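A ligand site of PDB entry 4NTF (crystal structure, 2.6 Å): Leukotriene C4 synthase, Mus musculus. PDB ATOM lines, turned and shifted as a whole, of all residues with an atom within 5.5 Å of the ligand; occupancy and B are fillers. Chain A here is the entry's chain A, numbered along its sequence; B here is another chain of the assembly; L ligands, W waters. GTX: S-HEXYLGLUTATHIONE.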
ATOM      1  N   ARG A  57      27.579 -10.310  33.757  1.00  0.00           N
ATOM      2  CA  ARG A  57      26.262 -10.050  33.237  1.00  0.00           C
ATOM      3  C   ARG A  57      26.290  -8.946  32.194  1.00  0.00           C
ATOM      4  O   ARG A  57      25.671  -9.053  31.123  1.00  0.00           O
ATOM      5  CB  ARG A  57      25.338  -9.682  34.400  1.00  0.00           C
ATOM      6  CG  ARG A  57      23.870  -9.698  34.076  1.00  0.00           C
ATOM      7  CD  ARG A  57      23.491 -10.957  33.356  1.00  0.00           C
ATOM      8  NE  ARG A  57      23.866 -12.180  34.058  1.00  0.00           N
ATOM      9  CZ  ARG A  57      23.914 -13.374  33.443  1.00  0.00           C
ATOM     10  NH1 ARG A  57      23.615 -13.459  32.138  1.00  0.00           N
ATOM     11  NH2 ARG A  57      24.248 -14.463  34.125  1.00  0.00           N
ATOM     12  N   ASN A  61      25.178  -9.441  28.246  1.00  0.00           N
ATOM     13  CA  ASN A  61      24.176  -8.571  27.694  1.00  0.00           C
ATOM     14  C   ASN A  61      24.642  -7.917  26.402  1.00  0.00           C
ATOM     15  O   ASN A  61      23.994  -8.006  25.352  1.00  0.00           O
ATOM     16  CB  ASN A  61      23.793  -7.545  28.731  1.00  0.00           C
ATOM     17  CG  ASN A  61      22.366  -7.656  29.132  1.00  0.00           C
ATOM     18  OD1 ASN A  61      21.507  -6.996  28.543  1.00  0.00           O
ATOM     19  ND2 ASN A  61      22.087  -8.540  30.102  1.00  0.00           N
ATOM     20  N   GLU A  64      24.750 -10.277  23.502  1.00  0.00           N
ATOM     21  CA  GLU A  64      23.612 -10.698  22.721  1.00  0.00           C
ATOM     22  C   GLU A  64      23.051  -9.525  21.933  1.00  0.00           C
ATOM     23  O   GLU A  64      22.432  -9.717  20.894  1.00  0.00           O
ATOM     24  CB  GLU A  64      22.559 -11.360  23.581  1.00  0.00           C
ATOM     25  CG  GLU A  64      22.020 -10.465  24.618  1.00  0.00           C
ATOM     26  CD  GLU A  64      20.956 -11.147  25.439  1.00  0.00           C
ATOM     27  OE1 GLU A  64      21.173 -12.338  25.791  1.00  0.00           O
ATOM     28  OE2 GLU A  64      19.919 -10.503  25.716  1.00  0.00           O
ATOM     29  N   TYR A  65      23.288  -8.310  22.372  1.00  0.00           N
ATOM     30  CA  TYR A  65      22.841  -7.193  21.567  1.00  0.00           C
ATOM     31  C   TYR A  65      23.734  -6.914  20.364  1.00  0.00           C
ATOM     32  O   TYR A  65      23.385  -6.157  19.457  1.00  0.00           O
ATOM     33  CB  TYR A  65      22.620  -5.952  22.411  1.00  0.00           C
ATOM     34  CG  TYR A  65      21.200  -5.913  22.829  1.00  0.00           C
ATOM     35  CD1 TYR A  65      20.246  -5.361  22.010  1.00  0.00           C
ATOM     36  CD2 TYR A  65      20.790  -6.507  24.022  1.00  0.00           C
ATOM     37  CE1 TYR A  65      18.939  -5.353  22.353  1.00  0.00           C
ATOM     38  CE2 TYR A  65      19.480  -6.501  24.394  1.00  0.00           C
ATOM     39  CZ  TYR A  65      18.552  -5.926  23.549  1.00  0.00           C
ATOM     40  OH  TYR A  65      17.220  -5.901  23.869  1.00  0.00           O
ATOM     41  N   LEU A  68      22.459  -7.814  16.899  1.00  0.00           N
ATOM     42  CA  LEU A  68      21.336  -6.980  16.522  1.00  0.00           C
ATOM     43  C   LEU A  68      21.931  -5.694  15.971  1.00  0.00           C
ATOM     44  O   LEU A  68      21.586  -5.246  14.887  1.00  0.00           O
ATOM     45  CB  LEU A  68      20.421  -6.683  17.692  1.00  0.00           C
ATOM     46  CG  LEU A  68      19.894  -7.869  18.510  1.00  0.00           C
ATOM     47  CD1 LEU A  68      18.693  -7.441  19.312  1.00  0.00           C
ATOM     48  CD2 LEU A  68      19.538  -9.052  17.623  1.00  0.00           C
ATOM     49  N   ARG A  96      27.049   1.536  25.078  1.00  0.00           N
ATOM     50  CA  ARG A  96      27.365   0.214  25.625  1.00  0.00           C
ATOM     51  C   ARG A  96      28.651   0.200  26.464  1.00  0.00           C
ATOM     52  O   ARG A  96      28.772  -0.576  27.420  1.00  0.00           O
ATOM     53  CB  ARG A  96      27.395  -0.850  24.535  1.00  0.00           C
ATOM     54  CG  ARG A  96      26.010  -1.274  24.040  1.00  0.00           C
ATOM     55  CD  ARG A  96      25.265  -2.069  25.079  1.00  0.00           C
ATOM     56  NE  ARG A  96      23.924  -2.393  24.620  1.00  0.00           N
ATOM     57  CZ  ARG A  96      23.165  -3.352  25.136  1.00  0.00           C
ATOM     58  NH1 ARG A  96      23.624  -4.105  26.133  1.00  0.00           N
ATOM     59  NH2 ARG A  96      21.947  -3.558  24.654  1.00  0.00           N
ATOM     60  N   TYR A  99      27.409   1.603  29.613  1.00  0.00           N
ATOM     61  CA  TYR A  99      26.596   0.525  30.172  1.00  0.00           C
ATOM     62  C   TYR A  99      27.449  -0.436  30.987  1.00  0.00           C
ATOM     63  O   TYR A  99      27.118  -0.760  32.125  1.00  0.00           O
ATOM     64  CB  TYR A  99      25.917  -0.267  29.054  1.00  0.00           C
ATOM     65  CG  TYR A  99      25.136  -1.477  29.521  1.00  0.00           C
ATOM     66  CD1 TYR A  99      23.885  -1.326  30.131  1.00  0.00           C
ATOM     67  CD2 TYR A  99      25.646  -2.756  29.381  1.00  0.00           C
ATOM     68  CE1 TYR A  99      23.158  -2.417  30.555  1.00  0.00           C
ATOM     69  CE2 TYR A  99      24.923  -3.874  29.820  1.00  0.00           C
ATOM     70  CZ  TYR A  99      23.676  -3.689  30.406  1.00  0.00           C
ATOM     71  OH  TYR A  99      22.965  -4.785  30.818  1.00  0.00           O
ATOM     72  N   TYR A 103      27.392  -0.891  35.054  1.00  0.00           N
ATOM     73  CA  TYR A 103      26.971  -2.178  35.578  1.00  0.00           C
ATOM     74  C   TYR A 103      28.016  -2.719  36.543  1.00  0.00           C
ATOM     75  O   TYR A 103      27.694  -3.187  37.649  1.00  0.00           O
ATOM     76  CB  TYR A 103      26.764  -3.167  34.421  1.00  0.00           C
ATOM     77  CG  TYR A 103      25.752  -4.245  34.725  1.00  0.00           C
ATOM     78  CD1 TYR A 103      25.355  -4.495  36.035  1.00  0.00           C
ATOM     79  CD2 TYR A 103      25.163  -4.997  33.707  1.00  0.00           C
ATOM     80  CE1 TYR A 103      24.429  -5.461  36.323  1.00  0.00           C
ATOM     81  CE2 TYR A 103      24.224  -5.975  33.983  1.00  0.00           C
ATOM     82  CZ  TYR A 103      23.870  -6.204  35.305  1.00  0.00           C
ATOM     83  OH  TYR A 103      22.941  -7.163  35.620  1.00  0.00           O
ATOM     84  N   ARG A 110      23.828   1.346  35.568  1.00  0.00           N
ATOM     85  CA  ARG A 110      23.807   0.801  34.229  1.00  0.00           C
ATOM     86  C   ARG A 110      22.599   1.296  33.424  1.00  0.00           C
ATOM     87  O   ARG A 110      22.617   1.265  32.187  1.00  0.00           O
ATOM     88  CB  ARG A 110      23.795  -0.729  34.302  1.00  0.00           C
ATOM     89  CG  ARG A 110      22.487  -1.383  33.828  1.00  0.00           C
ATOM     90  CD  ARG A 110      22.417  -2.850  34.187  1.00  0.00           C
ATOM     91  NE  ARG A 110      21.086  -3.412  33.966  1.00  0.00           N
ATOM     92  CZ  ARG A 110      20.054  -3.253  34.787  1.00  0.00           C
ATOM     93  NH1 ARG A 110      18.881  -3.806  34.497  1.00  0.00           N
ATOM     94  NH2 ARG A 110      20.195  -2.542  35.898  1.00  0.00           N
ATOM     95  N   LEU A 114      22.103   2.262  29.268  1.00  0.00           N
ATOM     96  CA  LEU A 114      21.269   1.248  28.656  1.00  0.00           C
ATOM     97  C   LEU A 114      20.188   1.936  27.837  1.00  0.00           C
ATOM     98  O   LEU A 114      19.943   1.588  26.687  1.00  0.00           O
ATOM     99  CB  LEU A 114      20.617   0.344  29.706  1.00  0.00           C
ATOM    100  CG  LEU A 114      19.588  -0.574  29.039  1.00  0.00           C
ATOM    101  CD1 LEU A 114      20.268  -1.438  27.970  1.00  0.00           C
ATOM    102  CD2 LEU A 114      18.824  -1.433  30.028  1.00  0.00           C
ATOM    103  N   ALA A 118      19.668   2.036  23.852  1.00  0.00           N
ATOM    104  CA  ALA A 118      18.455   1.510  23.233  1.00  0.00           C
ATOM    105  C   ALA A 118      17.957   2.504  22.193  1.00  0.00           C
ATOM    106  O   ALA A 118      17.697   2.124  21.035  1.00  0.00           O
ATOM    107  CB  ALA A 118      17.406   1.235  24.250  1.00  0.00           C
ATOM    108  N   LEU A 121      19.851   2.281  19.141  1.00  0.00           N
ATOM    109  CA  LEU A 121      19.611   1.018  18.450  1.00  0.00           C
ATOM    110  C   LEU A 121      18.251   1.071  17.771  1.00  0.00           C
ATOM    111  O   LEU A 121      18.081   0.579  16.653  1.00  0.00           O
ATOM    112  CB  LEU A 121      19.686  -0.131  19.442  1.00  0.00           C
ATOM    113  CG  LEU A 121      19.677  -1.542  18.852  1.00  0.00           C
ATOM    114  CD1 LEU A 121      20.534  -1.666  17.576  1.00  0.00           C
ATOM    115  CD2 LEU A 121      20.173  -2.505  19.928  1.00  0.00           C
ATOM    116  N   TRP A 122      17.293   1.720  18.430  1.00  0.00           N
ATOM    117  CA  TRP A 122      15.973   1.944  17.853  1.00  0.00           C
ATOM    118  C   TRP A 122      16.046   2.825  16.620  1.00  0.00           C
ATOM    119  O   TRP A 122      15.362   2.590  15.631  1.00  0.00           O
ATOM    120  CB  TRP A 122      15.048   2.558  18.888  1.00  0.00           C
ATOM    121  CG  TRP A 122      14.502   1.543  19.832  1.00  0.00           C
ATOM    122  CD1 TRP A 122      14.659   1.512  21.200  1.00  0.00           C
ATOM    123  CD2 TRP A 122      13.715   0.394  19.498  1.00  0.00           C
ATOM    124  NE1 TRP A 122      14.021   0.420  21.721  1.00  0.00           N
ATOM    125  CE2 TRP A 122      13.429  -0.281  20.696  1.00  0.00           C
ATOM    126  CE3 TRP A 122      13.233  -0.117  18.290  1.00  0.00           C
ATOM    127  CZ2 TRP A 122      12.677  -1.455  20.735  1.00  0.00           C
ATOM    128  CZ3 TRP A 122      12.481  -1.282  18.326  1.00  0.00           C
ATOM    129  CH2 TRP A 122      12.216  -1.933  19.541  1.00  0.00           C
ATOM    130  N   VAL A 125      17.213   0.888  13.697  1.00  0.00           N
ATOM    131  CA  VAL A 125      16.077   0.105  13.225  1.00  0.00           C
ATOM    132  C   VAL A 125      15.113   0.944  12.383  1.00  0.00           C
ATOM    133  O   VAL A 125      14.676   0.520  11.316  1.00  0.00           O
ATOM    134  CB  VAL A 125      15.339  -0.525  14.410  1.00  0.00           C
ATOM    135  CG1 VAL A 125      13.948  -0.996  14.009  1.00  0.00           C
ATOM    136  CG2 VAL A 125      16.181  -1.654  14.991  1.00  0.00           C
ATOM    137  N   VAL B  22      15.651  -9.108  13.655  1.00  0.00           N
ATOM    138  CA  VAL B  22      16.027  -8.157  14.691  1.00  0.00           C
ATOM    139  C   VAL B  22      14.808  -7.726  15.535  1.00  0.00           C
ATOM    140  O   VAL B  22      14.894  -7.656  16.757  1.00  0.00           O
ATOM    141  CB  VAL B  22      16.727  -6.896  14.084  1.00  0.00           C
ATOM    142  CG1 VAL B  22      16.904  -5.800  15.126  1.00  0.00           C
ATOM    143  CG2 VAL B  22      18.055  -7.256  13.452  1.00  0.00           C
ATOM    144  N   ALA B  26      14.194  -8.428  19.551  1.00  0.00           N
ATOM    145  CA  ALA B  26      13.883  -7.296  20.388  1.00  0.00           C
ATOM    146  C   ALA B  26      12.617  -7.610  21.158  1.00  0.00           C
ATOM    147  O   ALA B  26      12.485  -7.290  22.354  1.00  0.00           O
ATOM    148  CB  ALA B  26      13.695  -6.054  19.551  1.00  0.00           C
ATOM    149  N   SER B  29      13.412  -9.892  23.997  1.00  0.00           N
ATOM    150  CA  SER B  29      14.056  -9.117  25.043  1.00  0.00           C
ATOM    151  C   SER B  29      13.082  -8.368  25.946  1.00  0.00           C
ATOM    152  O   SER B  29      13.274  -8.306  27.173  1.00  0.00           O
ATOM    153  CB  SER B  29      15.027  -8.119  24.433  1.00  0.00           C
ATOM    154  OG  SER B  29      16.301  -8.705  24.289  1.00  0.00           O
ATOM    155  N   LEU B  30      12.048  -7.789  25.348  1.00  0.00           N
ATOM    156  CA  LEU B  30      11.083  -7.029  26.108  1.00  0.00           C
ATOM    157  C   LEU B  30      10.208  -7.983  26.906  1.00  0.00           C
ATOM    158  O   LEU B  30       9.772  -7.661  28.013  1.00  0.00           O
ATOM    159  CB  LEU B  30      10.274  -6.108  25.198  1.00  0.00           C
ATOM    160  CG  LEU B  30      11.083  -4.907  24.670  1.00  0.00           C
ATOM    161  CD1 LEU B  30      10.578  -4.439  23.306  1.00  0.00           C
ATOM    162  CD2 LEU B  30      11.110  -3.746  25.679  1.00  0.00           C
ATOM    163  N   VAL B  32      11.351 -10.691  28.232  1.00  0.00           N
ATOM    164  CA  VAL B  32      12.158 -11.003  29.389  1.00  0.00           C
ATOM    165  C   VAL B  32      12.087  -9.918  30.469  1.00  0.00           C
ATOM    166  O   VAL B  32      11.980 -10.240  31.643  1.00  0.00           O
ATOM    167  CB  VAL B  32      13.623 -11.314  29.015  1.00  0.00           C
ATOM    168  CG1 VAL B  32      14.504 -11.376  30.271  1.00  0.00           C
ATOM    169  CG2 VAL B  32      13.680 -12.618  28.269  1.00  0.00           C
ATOM    170  N   ILE B  33      12.135  -8.642  30.088  1.00  0.00           N
ATOM    171  CA  ILE B  33      11.954  -7.553  31.075  1.00  0.00           C
ATOM    172  C   ILE B  33      10.566  -7.656  31.707  1.00  0.00           C
ATOM    173  O   ILE B  33      10.384  -7.367  32.885  1.00  0.00           O
ATOM    174  CB  ILE B  33      12.087  -6.158  30.440  1.00  0.00           C
ATOM    175  CG1 ILE B  33      13.434  -5.991  29.764  1.00  0.00           C
ATOM    176  CG2 ILE B  33      11.907  -5.051  31.489  1.00  0.00           C
ATOM    177  CD1 ILE B  33      13.496  -4.674  29.085  1.00  0.00           C
ATOM    178  N   ARG B  36      10.843 -10.463  34.216  1.00  0.00           N
ATOM    179  CA  ARG B  36      11.659 -10.014  35.342  1.00  0.00           C
ATOM    180  C   ARG B  36      10.856  -9.231  36.385  1.00  0.00           C
ATOM    181  O   ARG B  36      11.054  -9.361  37.593  1.00  0.00           O
ATOM    182  CB  ARG B  36      12.834  -9.162  34.868  1.00  0.00           C
ATOM    183  CG  ARG B  36      13.996  -9.948  34.304  1.00  0.00           C
ATOM    184  CD  ARG B  36      15.285  -9.142  34.378  1.00  0.00           C
ATOM    185  NE  ARG B  36      16.429  -9.893  33.862  1.00  0.00           N
ATOM    186  CZ  ARG B  36      17.322 -10.544  34.607  1.00  0.00           C
ATOM    187  NH1 ARG B  36      17.201 -10.544  35.924  1.00  0.00           N
ATOM    188  NH2 ARG B  36      18.322 -11.184  34.030  1.00  0.00           N
ATOM    189  N   PRO B  43      18.247  -7.827  38.060  1.00  0.00           N
ATOM    190  CA  PRO B  43      19.634  -8.028  37.610  1.00  0.00           C
ATOM    191  C   PRO B  43      20.729  -7.880  38.709  1.00  0.00           C
ATOM    192  O   PRO B  43      20.635  -6.979  39.529  1.00  0.00           O
ATOM    193  CB  PRO B  43      19.795  -6.999  36.484  1.00  0.00           C
ATOM    194  CG  PRO B  43      18.403  -6.816  35.964  1.00  0.00           C
ATOM    195  CD  PRO B  43      17.521  -6.897  37.170  1.00  0.00           C
ATOM    196  N   THR B  46      19.760 -14.947  37.095  1.00  0.00           N
ATOM    197  CA  THR B  46      19.009 -15.419  35.945  1.00  0.00           C
ATOM    198  C   THR B  46      18.128 -16.577  36.380  1.00  0.00           C
ATOM    199  O   THR B  46      17.556 -17.311  35.543  1.00  0.00           O
ATOM    200  CB  THR B  46      19.967 -15.774  34.803  1.00  0.00           C
ATOM    201  OG1 THR B  46      20.846 -16.814  35.229  1.00  0.00           O
ATOM    202  CG2 THR B  46      20.785 -14.544  34.459  1.00  0.00           C
ATOM    203  N   PHE B  56      13.498 -16.656  30.212  1.00  0.00           N
ATOM    204  CA  PHE B  56      14.879 -16.236  30.050  1.00  0.00           C
ATOM    205  C   PHE B  56      15.567 -17.169  29.069  1.00  0.00           C
ATOM    206  O   PHE B  56      16.285 -16.734  28.152  1.00  0.00           O
ATOM    207  CB  PHE B  56      15.580 -16.267  31.398  1.00  0.00           C
ATOM    208  CG  PHE B  56      17.058 -16.101  31.325  1.00  0.00           C
ATOM    209  CD1 PHE B  56      17.636 -14.849  31.100  1.00  0.00           C
ATOM    210  CD2 PHE B  56      17.899 -17.186  31.502  1.00  0.00           C
ATOM    211  CE1 PHE B  56      19.013 -14.693  31.035  1.00  0.00           C
ATOM    212  CE2 PHE B  56      19.283 -17.032  31.431  1.00  0.00           C
ATOM    213  CZ  PHE B  56      19.838 -15.786  31.213  1.00  0.00           C
ATOM    214  N   GLN B  59      14.701 -16.877  25.335  1.00  0.00           N
ATOM    215  CA  GLN B  59      15.304 -15.690  24.731  1.00  0.00           C
ATOM    216  C   GLN B  59      16.762 -15.944  24.377  1.00  0.00           C
ATOM    217  O   GLN B  59      17.205 -15.622  23.266  1.00  0.00           O
ATOM    218  CB  GLN B  59      15.179 -14.476  25.658  1.00  0.00           C
ATOM    219  CG  GLN B  59      15.926 -13.221  25.197  1.00  0.00           C
ATOM    220  CD  GLN B  59      17.302 -13.045  25.843  1.00  0.00           C
ATOM    221  OE1 GLN B  59      17.420 -12.915  27.065  1.00  0.00           O
ATOM    222  NE2 GLN B  59      18.335 -13.023  25.037  1.00  0.00           N
ATOM    223  N   VAL B  60      17.469 -16.551  25.335  1.00  0.00           N
ATOM    224  CA  VAL B  60      18.884 -16.884  25.207  1.00  0.00           C
ATOM    225  C   VAL B  60      19.156 -17.818  24.059  1.00  0.00           C
ATOM    226  O   VAL B  60      20.073 -17.591  23.242  1.00  0.00           O
ATOM    227  CB  VAL B  60      19.414 -17.515  26.516  1.00  0.00           C
ATOM    228  CG1 VAL B  60      20.739 -18.261  26.297  1.00  0.00           C
ATOM    229  CG2 VAL B  60      19.535 -16.446  27.597  1.00  0.00           C
HETATM  230  N1  GTX L   1      19.043 -11.282  28.620  1.00  0.00           N
HETATM  231  CA1 GTX L   1      18.375 -10.104  29.099  1.00  0.00           C
HETATM  232  C1  GTX L   1      18.142 -10.109  30.591  1.00  0.00           C
HETATM  233  O11 GTX L   1      18.457 -11.120  31.286  1.00  0.00           O
HETATM  234  O12 GTX L   1      17.625  -9.105  31.163  1.00  0.00           O
HETATM  235  CB1 GTX L   1      17.074  -9.986  28.369  1.00  0.00           C
HETATM  236  CG1 GTX L   1      16.866  -8.908  27.385  1.00  0.00           C
HETATM  237  CD1 GTX L   1      17.166  -7.492  27.743  1.00  0.00           C
HETATM  238  OE1 GTX L   1      17.314  -7.180  28.916  1.00  0.00           O
HETATM  239  N2  GTX L   1      17.273  -6.532  26.690  1.00  0.00           N
HETATM  240  CA2 GTX L   1      17.566  -5.130  26.844  1.00  0.00           C
HETATM  241  C2  GTX L   1      18.736  -4.928  27.750  1.00  0.00           C
HETATM  242  O2  GTX L   1      19.798  -4.500  27.326  1.00  0.00           O
HETATM  243  CB2 GTX L   1      16.377  -4.364  27.329  1.00  0.00           C
HETATM  244  SG2 GTX L   1      15.129  -3.828  26.206  1.00  0.00           S
HETATM  245  C1S GTX L   1      15.508  -2.190  25.659  1.00  0.00           C
HETATM  246  C2S GTX L   1      15.937  -2.099  24.235  1.00  0.00           C
HETATM  247  C3S GTX L   1      15.381  -3.119  23.311  1.00  0.00           C
HETATM  248  C4S GTX L   1      16.101  -3.407  22.039  1.00  0.00           C
HETATM  249  C5S GTX L   1      16.114  -2.357  20.981  1.00  0.00           C
HETATM  250  C6S GTX L   1      16.201  -2.823  19.549  1.00  0.00           C
HETATM  251  N3  GTX L   1      18.582  -5.283  29.128  1.00  0.00           N
HETATM  252  CA3 GTX L   1      19.635  -5.148  30.094  1.00  0.00           C
HETATM  253  C3  GTX L   1      19.184  -5.517  31.447  1.00  0.00           C
HETATM  254  O31 GTX L   1      18.181  -4.920  31.903  1.00  0.00           O
HETATM  255  O32 GTX L   1      19.767  -6.442  32.084  1.00  0.00           O
HETATM  256  O   HOH W   1      21.227  -8.386  32.618  1.00  0.00           O
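An oxygen (O11) of the ligand is in salt-bridge range of the guanidinium group (NH2) of Arg 36 of chain B (2.7 Å).
A nitrogen (N1) of the ligand is in hydrogen-bond range of the side-chain amide oxygen (OE1) of Gln 59 of chain B (2.8 Å).
OH of Tyr 65 sits at hydrogen-bond distance from N2 of the ligand, 2.9 Å away.
NH1 of Arg 110 is in salt-bridge range of O31 of the ligand (2.9 Å).
The side-chain amide oxygen (OD1) of Asn 61 lies close to an oxygen (O2) of the ligand (3.3 Å).
N1 of the ligand lies within salt-bridge range of OE2 of Glu 64 (3.1 Å).
A nitrogen (N2) of the ligand sits close to the side-chain hydroxyl (OG) of Ser 29 of chain B (3.4 Å).
The side-chain carboxylate (OE1) of Glu 64 sits at hydrogen-bond distance from the side-chain amide nitrogen (NE2) of Gln 59 of chain B (3.0 Å).
The side-chain hydroxyl of Tyr 65 sits at hydrogen-bond distance from the side-chain hydroxyl of Ser 29 of chain B (3.0 Å).
OD1 of Asn 61 lies close to OH of Tyr 99 (3.5 Å).
Arg 96 touches the ligand (NH2 to O2, 3.6 Å).
Tyr 99 touches the ligand.
Leu 114 touches the ligand.
CB of Ala 118 touches C2S of the ligand, at 3.6 Å.
CG of Leu 121 touches C6S of the ligand, at 3.8 Å.
Trp 122 touches the ligand (CE2 to C5S, 3.4 Å).
Val 32 of chain B touches the ligand (CG1 to CB1, 3.5 Å).
Ile 33 of chain B touches the ligand (CD1 to CB2, 3.4 Å).
Phe 56 of chain B touches the ligand (CE1 to O11, 3.6 Å).
Hydrophobic or aromatic side chains that line the ligand: Tyr 65, Leu 114, Ala 118, Leu 121, Trp 122, Val 32 of chain B, Ile 33 of chain B and Phe 56 of chain B.
Of the 26 residues printed, 16 come within 4 Å of the ligand.
Water W1 lies within hydrogen-bond range of an oxygen (O32) of the ligand and the side-chain amide nitrogen (ND2) of Asn 61.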
